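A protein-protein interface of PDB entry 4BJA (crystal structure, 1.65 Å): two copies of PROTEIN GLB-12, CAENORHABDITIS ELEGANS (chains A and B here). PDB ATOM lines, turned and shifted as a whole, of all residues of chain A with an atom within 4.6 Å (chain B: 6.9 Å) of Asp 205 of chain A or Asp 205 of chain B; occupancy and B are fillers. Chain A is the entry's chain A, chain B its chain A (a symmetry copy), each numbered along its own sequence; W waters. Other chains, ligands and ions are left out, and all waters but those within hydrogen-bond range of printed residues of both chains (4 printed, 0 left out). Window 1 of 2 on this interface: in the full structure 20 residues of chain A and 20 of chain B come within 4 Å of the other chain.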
ATOM      1  N   TRP A  19     -15.298  -9.838  26.558  1.00  0.00           N
ATOM      2  CA  TRP A  19     -16.733  -9.565  26.870  1.00  0.00           C
ATOM      3  C   TRP A  19     -17.598 -10.593  26.218  1.00  0.00           C
ATOM      4  O   TRP A  19     -17.445 -10.888  25.021  1.00  0.00           O
ATOM      5  CB  TRP A  19     -17.179  -8.218  26.296  1.00  0.00           C
ATOM      6  CG  TRP A  19     -16.359  -7.067  26.758  1.00  0.00           C
ATOM      7  CD1 TRP A  19     -15.417  -6.394  26.032  1.00  0.00           C
ATOM      8  CD2 TRP A  19     -16.413  -6.439  28.040  1.00  0.00           C
ATOM      9  NE1 TRP A  19     -14.863  -5.394  26.796  1.00  0.00           N
ATOM     10  CE2 TRP A  19     -15.461  -5.396  28.033  1.00  0.00           C
ATOM     11  CE3 TRP A  19     -17.184  -6.646  29.200  1.00  0.00           C
ATOM     12  CZ2 TRP A  19     -15.247  -4.559  29.142  1.00  0.00           C
ATOM     13  CZ3 TRP A  19     -16.964  -5.826  30.301  1.00  0.00           C
ATOM     14  CH2 TRP A  19     -16.012  -4.787  30.262  1.00  0.00           C
ATOM     15  N   ARG A 121     -17.818  -6.112  17.978  1.00  0.00           N
ATOM     16  CA  ARG A 121     -16.562  -6.687  18.409  1.00  0.00           C
ATOM     17  C   ARG A 121     -16.151  -7.877  17.526  1.00  0.00           C
ATOM     18  O   ARG A 121     -14.973  -8.033  17.248  1.00  0.00           O
ATOM     19  CB  ARG A 121     -16.636  -7.022  19.901  1.00  0.00           C
ATOM     20  CG  ARG A 121     -16.747  -5.727  20.718  1.00  0.00           C
ATOM     21  CD  ARG A 121     -16.371  -5.850  22.150  1.00  0.00           C
ATOM     22  NE  ARG A 121     -14.986  -6.236  22.385  1.00  0.00           N
ATOM     23  CZ  ARG A 121     -14.019  -5.445  22.864  1.00  0.00           C
ATOM     24  NH1 ARG A 121     -14.203  -4.142  23.104  1.00  0.00           N
ATOM     25  NH2 ARG A 121     -12.838  -5.984  23.098  1.00  0.00           N
ATOM     26  N   SER A 201     -14.433   2.868  18.277  1.00  0.00           N
ATOM     27  CA  SER A 201     -13.688   2.452  19.466  1.00  0.00           C
ATOM     28  C   SER A 201     -13.792   0.927  19.676  1.00  0.00           C
ATOM     29  O   SER A 201     -12.790   0.291  20.012  1.00  0.00           O
ATOM     30  CB  SER A 201     -14.152   3.207  20.682  1.00  0.00           C
ATOM     31  OG  SER A 201     -15.426   2.775  21.035  1.00  0.00           O
ATOM     32  N   GLN A 202     -14.982   0.348  19.457  1.00  0.00           N
ATOM     33  CA  GLN A 202     -15.134  -1.089  19.732  1.00  0.00           C
ATOM     34  C   GLN A 202     -14.487  -1.954  18.666  1.00  0.00           C
ATOM     35  O   GLN A 202     -13.926  -3.017  18.984  1.00  0.00           O
ATOM     36  CB  GLN A 202     -16.613  -1.425  19.917  1.00  0.00           C
ATOM     37  CG  GLN A 202     -17.161  -0.682  21.139  1.00  0.00           C
ATOM     38  CD  GLN A 202     -16.322  -0.989  22.385  1.00  0.00           C
ATOM     39  OE1 GLN A 202     -16.302  -2.121  22.852  1.00  0.00           O
ATOM     40  NE2 GLN A 202     -15.572   0.015  22.888  1.00  0.00           N
ATOM     41  N   MET A 203     -14.504  -1.491  17.407  1.00  0.00           N
ATOM     42  CA  MET A 203     -13.762  -2.251  16.404  1.00  0.00           C
ATOM     43  C   MET A 203     -12.277  -2.124  16.637  1.00  0.00           C
ATOM     44  O   MET A 203     -11.561  -3.111  16.509  1.00  0.00           O
ATOM     45  CB  MET A 203     -14.126  -1.831  14.996  1.00  0.00           C
ATOM     46  CG  MET A 203     -15.521  -2.250  14.631  1.00  0.00           C
ATOM     47  SD  MET A 203     -15.885  -1.651  12.994  1.00  0.00           S
ATOM     48  CE  MET A 203     -14.937  -2.802  12.025  1.00  0.00           C
ATOM     49  N   THR A 204     -11.818  -0.940  17.028  1.00  0.00           N
ATOM     50  CA  THR A 204     -10.414  -0.756  17.280  1.00  0.00           C
ATOM     51  C   THR A 204      -9.935  -1.641  18.438  1.00  0.00           C
ATOM     52  O   THR A 204      -8.878  -2.293  18.334  1.00  0.00           O
ATOM     53  CB  THR A 204     -10.131   0.728  17.569  1.00  0.00           C
ATOM     54  OG1 THR A 204     -10.430   1.487  16.388  1.00  0.00           O
ATOM     55  CG2 THR A 204      -8.678   0.946  18.012  1.00  0.00           C
ATOM     56  N   ASP A 205     -10.708  -1.650  19.531  1.00  0.00           N
ATOM     57  CA  ASP A 205     -10.283  -2.377  20.722  1.00  0.00           C
ATOM     58  C   ASP A 205     -10.322  -3.875  20.518  1.00  0.00           C
ATOM     59  O   ASP A 205      -9.387  -4.574  20.918  1.00  0.00           O
ATOM     60  CB  ASP A 205     -11.096  -1.940  21.944  1.00  0.00           C
ATOM     61  CG  ASP A 205     -10.612  -0.611  22.533  1.00  0.00           C
ATOM     62  OD1 ASP A 205      -9.593  -0.037  22.072  1.00  0.00           O
ATOM     63  OD2 ASP A 205     -11.244  -0.137  23.506  1.00  0.00           O
ATOM     64  N   SER A 206     -11.373  -4.352  19.845  1.00  0.00           N
ATOM     65  CA  SER A 206     -11.484  -5.772  19.611  1.00  0.00           C
ATOM     66  C   SER A 206     -10.393  -6.266  18.636  1.00  0.00           C
ATOM     67  O   SER A 206      -9.757  -7.337  18.829  1.00  0.00           O
ATOM     68  CB  SER A 206     -12.890  -6.127  19.156  1.00  0.00           C
ATOM     69  OG  SER A 206     -13.251  -5.466  17.941  1.00  0.00           O
ATOM     70  N   PHE A 207     -10.165  -5.486  17.593  1.00  0.00           N
ATOM     71  CA  PHE A 207      -9.060  -5.787  16.684  1.00  0.00           C
ATOM     72  C   PHE A 207      -7.700  -5.863  17.434  1.00  0.00           C
ATOM     73  O   PHE A 207      -6.888  -6.793  17.242  1.00  0.00           O
ATOM     74  CB  PHE A 207      -9.013  -4.701  15.580  1.00  0.00           C
ATOM     75  CG  PHE A 207      -7.905  -4.923  14.573  1.00  0.00           C
ATOM     76  CD1 PHE A 207      -6.597  -4.549  14.873  1.00  0.00           C
ATOM     77  CD2 PHE A 207      -8.177  -5.541  13.362  1.00  0.00           C
ATOM     78  CE1 PHE A 207      -5.548  -4.800  13.965  1.00  0.00           C
ATOM     79  CE2 PHE A 207      -7.127  -5.755  12.421  1.00  0.00           C
ATOM     80  CZ  PHE A 207      -5.838  -5.414  12.748  1.00  0.00           C
ATOM     81  N   GLU A 208      -7.430  -4.861  18.266  1.00  0.00           N
ATOM     82  CA  GLU A 208      -6.127  -4.739  18.869  1.00  0.00           C
ATOM     83  C   GLU A 208      -5.869  -5.951  19.774  1.00  0.00           C
ATOM     84  O   GLU A 208      -4.766  -6.527  19.778  1.00  0.00           O
ATOM     85  CB  GLU A 208      -6.058  -3.436  19.627  1.00  0.00           C
ATOM     86  CG  GLU A 208      -4.678  -2.982  19.936  1.00  0.00           C
ATOM     87  CD  GLU A 208      -3.900  -2.484  18.707  1.00  0.00           C
ATOM     88  OE1 GLU A 208      -4.493  -1.911  17.767  1.00  0.00           O
ATOM     89  OE2 GLU A 208      -2.672  -2.640  18.719  1.00  0.00           O
ATOM     90  N   LEU A 209      -6.896  -6.338  20.510  1.00  0.00           N
ATOM     91  CA  LEU A 209      -6.782  -7.472  21.434  1.00  0.00           C
ATOM     92  C   LEU A 209      -6.571  -8.777  20.671  1.00  0.00           C
ATOM     93  O   LEU A 209      -5.747  -9.614  21.067  1.00  0.00           O
ATOM     94  CB  LEU A 209      -8.047  -7.561  22.293  1.00  0.00           C
ATOM     95  CG  LEU A 209      -8.040  -8.691  23.351  1.00  0.00           C
ATOM     96  CD1 LEU A 209      -6.853  -8.579  24.294  1.00  0.00           C
ATOM     97  CD2 LEU A 209      -9.350  -8.674  24.163  1.00  0.00           C
ATOM     98  N   TRP B  19      -4.507   3.676  22.274  1.00  0.00           N
ATOM     99  CA  TRP B  19      -5.044   5.069  22.252  1.00  0.00           C
ATOM    100  C   TRP B  19      -4.065   6.001  22.886  1.00  0.00           C
ATOM    101  O   TRP B  19      -3.551   5.733  23.985  1.00  0.00           O
ATOM    102  CB  TRP B  19      -6.327   5.183  23.079  1.00  0.00           C
ATOM    103  CG  TRP B  19      -7.401   4.247  22.655  1.00  0.00           C
ATOM    104  CD1 TRP B  19      -7.790   3.107  23.299  1.00  0.00           C
ATOM    105  CD2 TRP B  19      -8.238   4.372  21.504  1.00  0.00           C
ATOM    106  NE1 TRP B  19      -8.808   2.499  22.604  1.00  0.00           N
ATOM    107  CE2 TRP B  19      -9.108   3.259  21.498  1.00  0.00           C
ATOM    108  CE3 TRP B  19      -8.350   5.325  20.474  1.00  0.00           C
ATOM    109  CZ2 TRP B  19     -10.078   3.061  20.501  1.00  0.00           C
ATOM    110  CZ3 TRP B  19      -9.302   5.123  19.481  1.00  0.00           C
ATOM    111  CH2 TRP B  19     -10.162   4.007  19.506  1.00  0.00           C
ATOM    112  N   TRP B 117      -9.369   9.963  30.433  1.00  0.00           N
ATOM    113  CA  TRP B 117      -9.284   8.661  29.760  1.00  0.00           C
ATOM    114  C   TRP B 117      -7.914   8.026  29.940  1.00  0.00           C
ATOM    115  O   TRP B 117      -7.780   6.808  30.209  1.00  0.00           O
ATOM    116  CB  TRP B 117      -9.680   8.858  28.280  1.00  0.00           C
ATOM    117  CG  TRP B 117      -9.943   7.606  27.526  1.00  0.00           C
ATOM    118  CD1 TRP B 117     -10.336   6.357  28.020  1.00  0.00           C
ATOM    119  CD2 TRP B 117      -9.909   7.483  26.111  1.00  0.00           C
ATOM    120  NE1 TRP B 117     -10.517   5.483  26.961  1.00  0.00           N
ATOM    121  CE2 TRP B 117     -10.245   6.148  25.786  1.00  0.00           C
ATOM    122  CE3 TRP B 117      -9.606   8.386  25.077  1.00  0.00           C
ATOM    123  CZ2 TRP B 117     -10.314   5.691  24.458  1.00  0.00           C
ATOM    124  CZ3 TRP B 117      -9.667   7.916  23.742  1.00  0.00           C
ATOM    125  CH2 TRP B 117     -10.019   6.586  23.461  1.00  0.00           C
ATOM    126  N   ARG B 121      -7.065   4.241  31.600  1.00  0.00           N
ATOM    127  CA  ARG B 121      -6.387   3.181  30.885  1.00  0.00           C
ATOM    128  C   ARG B 121      -5.016   2.865  31.505  1.00  0.00           C
ATOM    129  O   ARG B 121      -4.638   1.706  31.555  1.00  0.00           O
ATOM    130  CB  ARG B 121      -6.325   3.527  29.394  1.00  0.00           C
ATOM    131  CG  ARG B 121      -7.742   3.522  28.802  1.00  0.00           C
ATOM    132  CD  ARG B 121      -7.807   3.383  27.325  1.00  0.00           C
ATOM    133  NE  ARG B 121      -7.260   2.137  26.805  1.00  0.00           N
ATOM    134  CZ  ARG B 121      -7.964   1.124  26.288  1.00  0.00           C
ATOM    135  NH1 ARG B 121      -9.302   1.106  26.271  1.00  0.00           N
ATOM    136  NH2 ARG B 121      -7.299   0.103  25.782  1.00  0.00           N
ATOM    137  N   GLY B 124      -5.671   0.726  34.492  1.00  0.00           N
ATOM    138  CA  GLY B 124      -5.992  -0.630  34.026  1.00  0.00           C
ATOM    139  C   GLY B 124      -4.725  -1.416  33.673  1.00  0.00           C
ATOM    140  O   GLY B 124      -4.514  -2.560  34.136  1.00  0.00           O
ATOM    141  N   ARG B 125      -3.849  -0.804  32.872  1.00  0.00           N
ATOM    142  CA  ARG B 125      -2.599  -1.454  32.471  1.00  0.00           C
ATOM    143  C   ARG B 125      -1.709  -1.782  33.658  1.00  0.00           C
ATOM    144  O   ARG B 125      -1.066  -2.834  33.661  1.00  0.00           O
ATOM    145  CB  ARG B 125      -1.797  -0.546  31.493  1.00  0.00           C
ATOM    146  CG  ARG B 125      -2.529  -0.278  30.183  1.00  0.00           C
ATOM    147  CD  ARG B 125      -1.570   0.272  29.096  1.00  0.00           C
ATOM    148  NE  ARG B 125      -0.774   1.382  29.608  1.00  0.00           N
ATOM    149  CZ  ARG B 125      -1.146   2.662  29.578  1.00  0.00           C
ATOM    150  NH1 ARG B 125      -2.317   3.024  29.051  1.00  0.00           N
ATOM    151  NH2 ARG B 125      -0.330   3.596  30.065  1.00  0.00           N
ATOM    152  N   GLN B 139     -12.913 -12.224  32.070  1.00  0.00           N
ATOM    153  CA  GLN B 139     -14.240 -11.777  31.606  1.00  0.00           C
ATOM    154  C   GLN B 139     -15.311 -12.898  31.432  1.00  0.00           C
ATOM    155  O   GLN B 139     -16.520 -12.623  31.365  1.00  0.00           O
ATOM    156  CB  GLN B 139     -14.072 -10.978  30.299  1.00  0.00           C
ATOM    157  CG  GLN B 139     -12.981  -9.866  30.356  1.00  0.00           C
ATOM    158  CD  GLN B 139     -13.009  -8.975  29.111  1.00  0.00           C
ATOM    159  OE1 GLN B 139     -11.989  -8.737  28.450  1.00  0.00           O
ATOM    160  NE2 GLN B 139     -14.183  -8.487  28.793  1.00  0.00           N
ATOM    161  N   ASN B 143     -14.711 -10.783  36.671  1.00  0.00           N
ATOM    162  CA  ASN B 143     -14.024  -9.523  36.357  1.00  0.00           C
ATOM    163  C   ASN B 143     -13.923  -8.717  37.657  1.00  0.00           C
ATOM    164  O   ASN B 143     -14.918  -8.204  38.127  1.00  0.00           O
ATOM    165  CB  ASN B 143     -14.845  -8.769  35.294  1.00  0.00           C
ATOM    166  CG  ASN B 143     -14.257  -7.432  34.951  1.00  0.00           C
ATOM    167  OD1 ASN B 143     -13.516  -6.844  35.739  1.00  0.00           O
ATOM    168  ND2 ASN B 143     -14.554  -6.953  33.738  1.00  0.00           N
ATOM    169  N   PHE B 145     -12.523  -5.864  38.419  1.00  0.00           N
ATOM    170  CA  PHE B 145     -12.819  -4.450  38.368  1.00  0.00           C
ATOM    171  C   PHE B 145     -14.312  -4.240  38.439  1.00  0.00           C
ATOM    172  O   PHE B 145     -14.796  -3.320  39.123  1.00  0.00           O
ATOM    173  CB  PHE B 145     -12.286  -3.853  37.055  1.00  0.00           C
ATOM    174  CG  PHE B 145     -10.809  -4.054  36.872  1.00  0.00           C
ATOM    175  CD1 PHE B 145      -9.920  -3.683  37.899  1.00  0.00           C
ATOM    176  CD2 PHE B 145     -10.322  -4.700  35.729  1.00  0.00           C
ATOM    177  CE1 PHE B 145      -8.535  -3.891  37.720  1.00  0.00           C
ATOM    178  CE2 PHE B 145      -8.964  -4.914  35.563  1.00  0.00           C
ATOM    179  CZ  PHE B 145      -8.075  -4.512  36.562  1.00  0.00           C
ATOM    180  N   VAL B 199     -15.756   3.415  33.668  1.00  0.00           N
ATOM    181  CA  VAL B 199     -14.503   3.102  34.328  1.00  0.00           C
ATOM    182  C   VAL B 199     -14.234   1.588  34.274  1.00  0.00           C
ATOM    183  O   VAL B 199     -13.138   1.140  33.917  1.00  0.00           O
ATOM    184  CB  VAL B 199     -14.498   3.615  35.781  1.00  0.00           C
ATOM    185  CG1 VAL B 199     -13.266   3.079  36.512  1.00  0.00           C
ATOM    186  CG2 VAL B 199     -14.539   5.203  35.763  1.00  0.00           C
ATOM    187  N   ILE B 200     -15.258   0.787  34.551  1.00  0.00           N
ATOM    188  CA  ILE B 200     -15.081  -0.676  34.453  1.00  0.00           C
ATOM    189  C   ILE B 200     -14.646  -1.088  33.050  1.00  0.00           C
ATOM    190  O   ILE B 200     -13.693  -1.836  32.891  1.00  0.00           O
ATOM    191  CB  ILE B 200     -16.382  -1.425  34.758  1.00  0.00           C
ATOM    192  CG1 ILE B 200     -16.755  -1.224  36.224  1.00  0.00           C
ATOM    193  CG2 ILE B 200     -16.165  -2.953  34.501  1.00  0.00           C
ATOM    194  CD1 ILE B 200     -18.221  -1.684  36.572  1.00  0.00           C
ATOM    195  N   SER B 201     -15.344  -0.603  32.021  1.00  0.00           N
ATOM    196  CA  SER B 201     -15.028  -1.084  30.675  1.00  0.00           C
ATOM    197  C   SER B 201     -13.594  -0.683  30.270  1.00  0.00           C
ATOM    198  O   SER B 201     -12.880  -1.498  29.682  1.00  0.00           O
ATOM    199  CB  SER B 201     -16.040  -0.592  29.676  1.00  0.00           C
ATOM    200  OG  SER B 201     -15.872   0.775  29.486  1.00  0.00           O
ATOM    201  N   GLN B 202     -13.174   0.547  30.602  1.00  0.00           N
ATOM    202  CA  GLN B 202     -11.845   0.989  30.154  1.00  0.00           C
ATOM    203  C   GLN B 202     -10.724   0.360  30.960  1.00  0.00           C
ATOM    204  O   GLN B 202      -9.656   0.047  30.403  1.00  0.00           O
ATOM    205  CB  GLN B 202     -11.775   2.516  30.176  1.00  0.00           C
ATOM    206  CG  GLN B 202     -12.788   3.092  29.184  1.00  0.00           C
ATOM    207  CD  GLN B 202     -12.573   2.508  27.783  1.00  0.00           C
ATOM    208  OE1 GLN B 202     -11.547   2.756  27.162  1.00  0.00           O
ATOM    209  NE2 GLN B 202     -13.521   1.672  27.310  1.00  0.00           N
ATOM    210  N   MET B 203     -10.963   0.114  32.257  1.00  0.00           N
ATOM    211  CA  MET B 203      -9.940  -0.618  33.001  1.00  0.00           C
ATOM    212  C   MET B 203      -9.878  -2.052  32.539  1.00  0.00           C
ATOM    213  O   MET B 203      -8.786  -2.593  32.401  1.00  0.00           O
ATOM    214  CB  MET B 203     -10.166  -0.539  34.495  1.00  0.00           C
ATOM    215  CG  MET B 203      -9.908   0.841  35.027  1.00  0.00           C
ATOM    216  SD  MET B 203     -10.270   0.855  36.771  1.00  0.00           S
ATOM    217  CE  MET B 203      -8.840  -0.003  37.391  1.00  0.00           C
ATOM    218  N   THR B 204     -11.027  -2.654  32.250  1.00  0.00           N
ATOM    219  CA  THR B 204     -11.035  -4.017  31.793  1.00  0.00           C
ATOM    220  C   THR B 204     -10.297  -4.161  30.455  1.00  0.00           C
ATOM    221  O   THR B 204      -9.484  -5.090  30.285  1.00  0.00           O
ATOM    222  CB  THR B 204     -12.486  -4.515  31.676  1.00  0.00           C
ATOM    223  OG1 THR B 204     -13.070  -4.527  32.987  1.00  0.00           O
ATOM    224  CG2 THR B 204     -12.553  -5.904  31.029  1.00  0.00           C
ATOM    225  N   ASP B 205     -10.591  -3.250  29.520  1.00  0.00           N
ATOM    226  CA  ASP B 205     -10.020  -3.365  28.182  1.00  0.00           C
ATOM    227  C   ASP B 205      -8.533  -3.091  28.173  1.00  0.00           C
ATOM    228  O   ASP B 205      -7.778  -3.820  27.524  1.00  0.00           O
ATOM    229  CB  ASP B 205     -10.776  -2.475  27.191  1.00  0.00           C
ATOM    230  CG  ASP B 205     -12.097  -3.097  26.726  1.00  0.00           C
ATOM    231  OD1 ASP B 205     -12.422  -4.258  27.084  1.00  0.00           O
ATOM    232  OD2 ASP B 205     -12.820  -2.427  25.951  1.00  0.00           O
ATOM    233  N   SER B 206      -8.115  -2.079  28.940  1.00  0.00           N
ATOM    234  CA  SER B 206      -6.709  -1.753  28.982  1.00  0.00           C
ATOM    235  C   SER B 206      -5.897  -2.868  29.678  1.00  0.00           C
ATOM    236  O   SER B 206      -4.790  -3.269  29.229  1.00  0.00           O
ATOM    237  CB  SER B 206      -6.500  -0.387  29.614  1.00  0.00           C
ATOM    238  OG  SER B 206      -6.993  -0.326  30.954  1.00  0.00           O
ATOM    239  N   PHE B 207      -6.445  -3.377  30.768  1.00  0.00           N
ATOM    240  CA  PHE B 207      -5.830  -4.530  31.424  1.00  0.00           C
ATOM    241  C   PHE B 207      -5.676  -5.733  30.451  1.00  0.00           C
ATOM    242  O   PHE B 207      -4.614  -6.387  30.368  1.00  0.00           O
ATOM    243  CB  PHE B 207      -6.692  -4.926  32.648  1.00  0.00           C
ATOM    244  CG  PHE B 207      -6.138  -6.110  33.411  1.00  0.00           C
ATOM    245  CD1 PHE B 207      -6.353  -7.407  32.950  1.00  0.00           C
ATOM    246  CD2 PHE B 207      -5.372  -5.909  34.549  1.00  0.00           C
ATOM    247  CE1 PHE B 207      -5.796  -8.514  33.621  1.00  0.00           C
ATOM    248  CE2 PHE B 207      -4.844  -7.028  35.258  1.00  0.00           C
ATOM    249  CZ  PHE B 207      -5.035  -8.297  34.769  1.00  0.00           C
ATOM    250  N   GLU B 208      -6.751  -6.055  29.737  1.00  0.00           N
ATOM    251  CA  GLU B 208      -6.774  -7.258  28.946  1.00  0.00           C
ATOM    252  C   GLU B 208      -5.707  -7.166  27.846  1.00  0.00           C
ATOM    253  O   GLU B 208      -4.979  -8.137  27.573  1.00  0.00           O
ATOM    254  CB  GLU B 208      -8.161  -7.448  28.382  1.00  0.00           C
ATOM    255  CG  GLU B 208      -8.445  -8.827  27.912  1.00  0.00           C
ATOM    256  CD  GLU B 208      -8.603  -9.849  29.050  1.00  0.00           C
ATOM    257  OE1 GLU B 208      -9.092  -9.508  30.149  1.00  0.00           O
ATOM    258  OE2 GLU B 208      -8.266 -11.016  28.808  1.00  0.00           O
ATOM    259  N   LEU B 209      -5.612  -5.991  27.247  1.00  0.00           N
ATOM    260  CA  LEU B 209      -4.647  -5.769  26.165  1.00  0.00           C
ATOM    261  C   LEU B 209      -3.215  -5.853  26.686  1.00  0.00           C
ATOM    262  O   LEU B 209      -2.341  -6.451  26.041  1.00  0.00           O
ATOM    263  CB  LEU B 209      -4.899  -4.399  25.529  1.00  0.00           C
ATOM    264  CG  LEU B 209      -3.976  -4.054  24.334  1.00  0.00           C
ATOM    265  CD1 LEU B 209      -4.064  -5.094  23.230  1.00  0.00           C
ATOM    266  CD2 LEU B 209      -4.330  -2.665  23.768  1.00  0.00           C
ATOM    267  N   GLU B 210      -2.970  -5.219  27.829  1.00  0.00           N
ATOM    268  CA  GLU B 210      -1.638  -5.201  28.390  1.00  0.00           C
ATOM    269  C   GLU B 210      -1.199  -6.607  28.786  1.00  0.00           C
ATOM    270  O   GLU B 210      -0.034  -7.000  28.549  1.00  0.00           O
ATOM    271  CB  GLU B 210      -1.578  -4.254  29.581  1.00  0.00           C
ATOM    272  CG  GLU B 210      -0.200  -4.213  30.290  1.00  0.00           C
ATOM    273  CD  GLU B 210       0.902  -3.584  29.432  1.00  0.00           C
ATOM    274  OE1 GLU B 210       0.609  -2.860  28.457  1.00  0.00           O
ATOM    275  OE2 GLU B 210       2.087  -3.800  29.758  1.00  0.00           O
HETATM  276  O   HOH W   1     -14.899   2.803  24.540  1.00  0.00           O
HETATM  277  O   HOH W   2     -15.480  -1.831  25.955  1.00  0.00           O
HETATM  278  O   HOH W   3     -12.230   2.348  24.039  1.00  0.00           O
HETATM  279  O   HOH W   4     -16.414   0.760  25.984  1.00  0.00           O
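Of the printed residues of chain B, Ser 201 of chain A touches Trp 19 (3.8 Å). Ser 206 of chain A touches none of the printed residues of chain B. Of the printed residues of chain B, Glu 208 of chain A touches Leu 209. Of the printed residues of chain A, Arg 121 of chain B touches Asp 205. Printed residues of chain A within 4 Å of Ser 201 of chain B: Trp 19 (3.8 Å). Of the printed residues of chain A, Asp 205 of chain B touches Trp 19, Arg 121 and Asp 205. Printed residues of chain A within 4 Å of Leu 209 of chain B: Glu 208. The nearest printed residue of chain A that does not touch Asp 205 of chain B is Gln 202 of chain A (4.7 Å). The nearest printed residue of chain A that does not touch Trp 19 of chain B is Gln 202 of chain A (5.7 Å).
The backbone NH (N) of Trp 19 of chain A lies close to the side-chain amide nitrogen (NE2) of Gln 139 of chain B, at 2.8 Å. The guanidinium group of Arg 121 of chain A is in salt-bridge range of the side-chain carboxylate of Asp 205 of chain B (3.6 Å). The indole nitrogen of Trp 19 of chain A sits at hydrogen-bond distance from the side-chain carboxylate of Asp 205 of chain B. The indole nitrogen of Trp 19 of chain B sits at hydrogen-bond distance from the side-chain carboxylate of Asp 205 of chain A, at 2.7 Å. OD2 of Asp 205 of chain A is in salt-bridge range of NH1 of Arg 121 of chain B (3.6 Å).
Among the printed residues, pairs that only touch across the chains: Trp 19 of chain A with Ser 201 of chain B (3.8 Å), Trp 19 of chain A with Thr 204 of chain B (3.6 Å), Ser 201 of chain A with Trp 19 of chain B (3.8 Å), Thr 204 of chain A with Trp 19 of chain B (3.6 Å), Asp 205 of chain A with Asp 205 of chain B (3.7 Å), Glu 208 of chain A with Leu 209 of chain B (3.8 Å) and Leu 209 of chain A with Glu 208 of chain B (3.8 Å).
Trp 19 of chain A touches Asp 205 of chain B, and with the chains exchanged Asp 205 of chain A touches Trp 19 of chain B. Arg 121 of chain A touches Asp 205 of chain B, and with the chains exchanged Asp 205 of chain A touches Arg 121 of chain B. Asp 205 of chain A touches its own counterpart, Asp 205 of chain B. Glu 208 of chain A touches Leu 209 of chain B, and with the chains exchanged Leu 209 of chain A touches Glu 208 of chain B.
Along chain B the printed residues that touch a printed residue of chain A span positions 19 to 209. Among the printed residues, Asp or Glu carboxylates within 4 Å of a Lys or Arg side-chain nitrogen of the other chain: Arg 121 of chain A with Asp 205 of chain B (3.6 Å) and Asp 205 of chain A with Arg 121 of chain B (3.6 Å).
Water W3 lies within hydrogen-bond range of the side-chain carboxylate (OD2) of Asp 205 of chain A (2.7 Å) and the side-chain amide oxygen (OE1) of Gln 202 of chain B (3.2 Å). Water W2 lies within hydrogen-bond range of the side-chain carboxylate (OD2) of Asp 205 of chain B (2.7 Å) and the side-chain amide oxygen (OE1) of Gln 202 of chain A (3.2 Å). Water W1 bridges NE2 of Gln 202 of chain B (3.3 Å) and NE2 of Gln 202 of chain A (3.3 Å). Water W4 lies within hydrogen-bond range of NE2 of Gln 202 of chain A (3.3 Å) and NE2 of Gln 202 of chain B (3.3 Å).
OE1 of Gln 202 of chain A is in hydrogen-bond range of NH1 of Arg 121 of chain A (2.9 Å). OG1 of Thr 204 of chain B sits at hydrogen-bond distance from O of Ile 200 of chain B (2.8 Å). The side-chain hydroxyl (OG) of Ser 201 of chain B lies within hydrogen-bond range of the side-chain amide nitrogen (NE2) of Gln 202 of chain B (3.3 Å). NE2 of Gln 202 of chain A is in hydrogen-bond range of OG of Ser 201 of chain A (3.3 Å). The side-chain amide oxygen (OE1) of Gln 202 of chain B sits at hydrogen-bond distance from the guanidinium group (NH1) of Arg 121 of chain B (2.9 Å). O of Arg 121 of chain A lies within hydrogen-bond range of OG of Ser 206 of chain A (3.2 Å).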
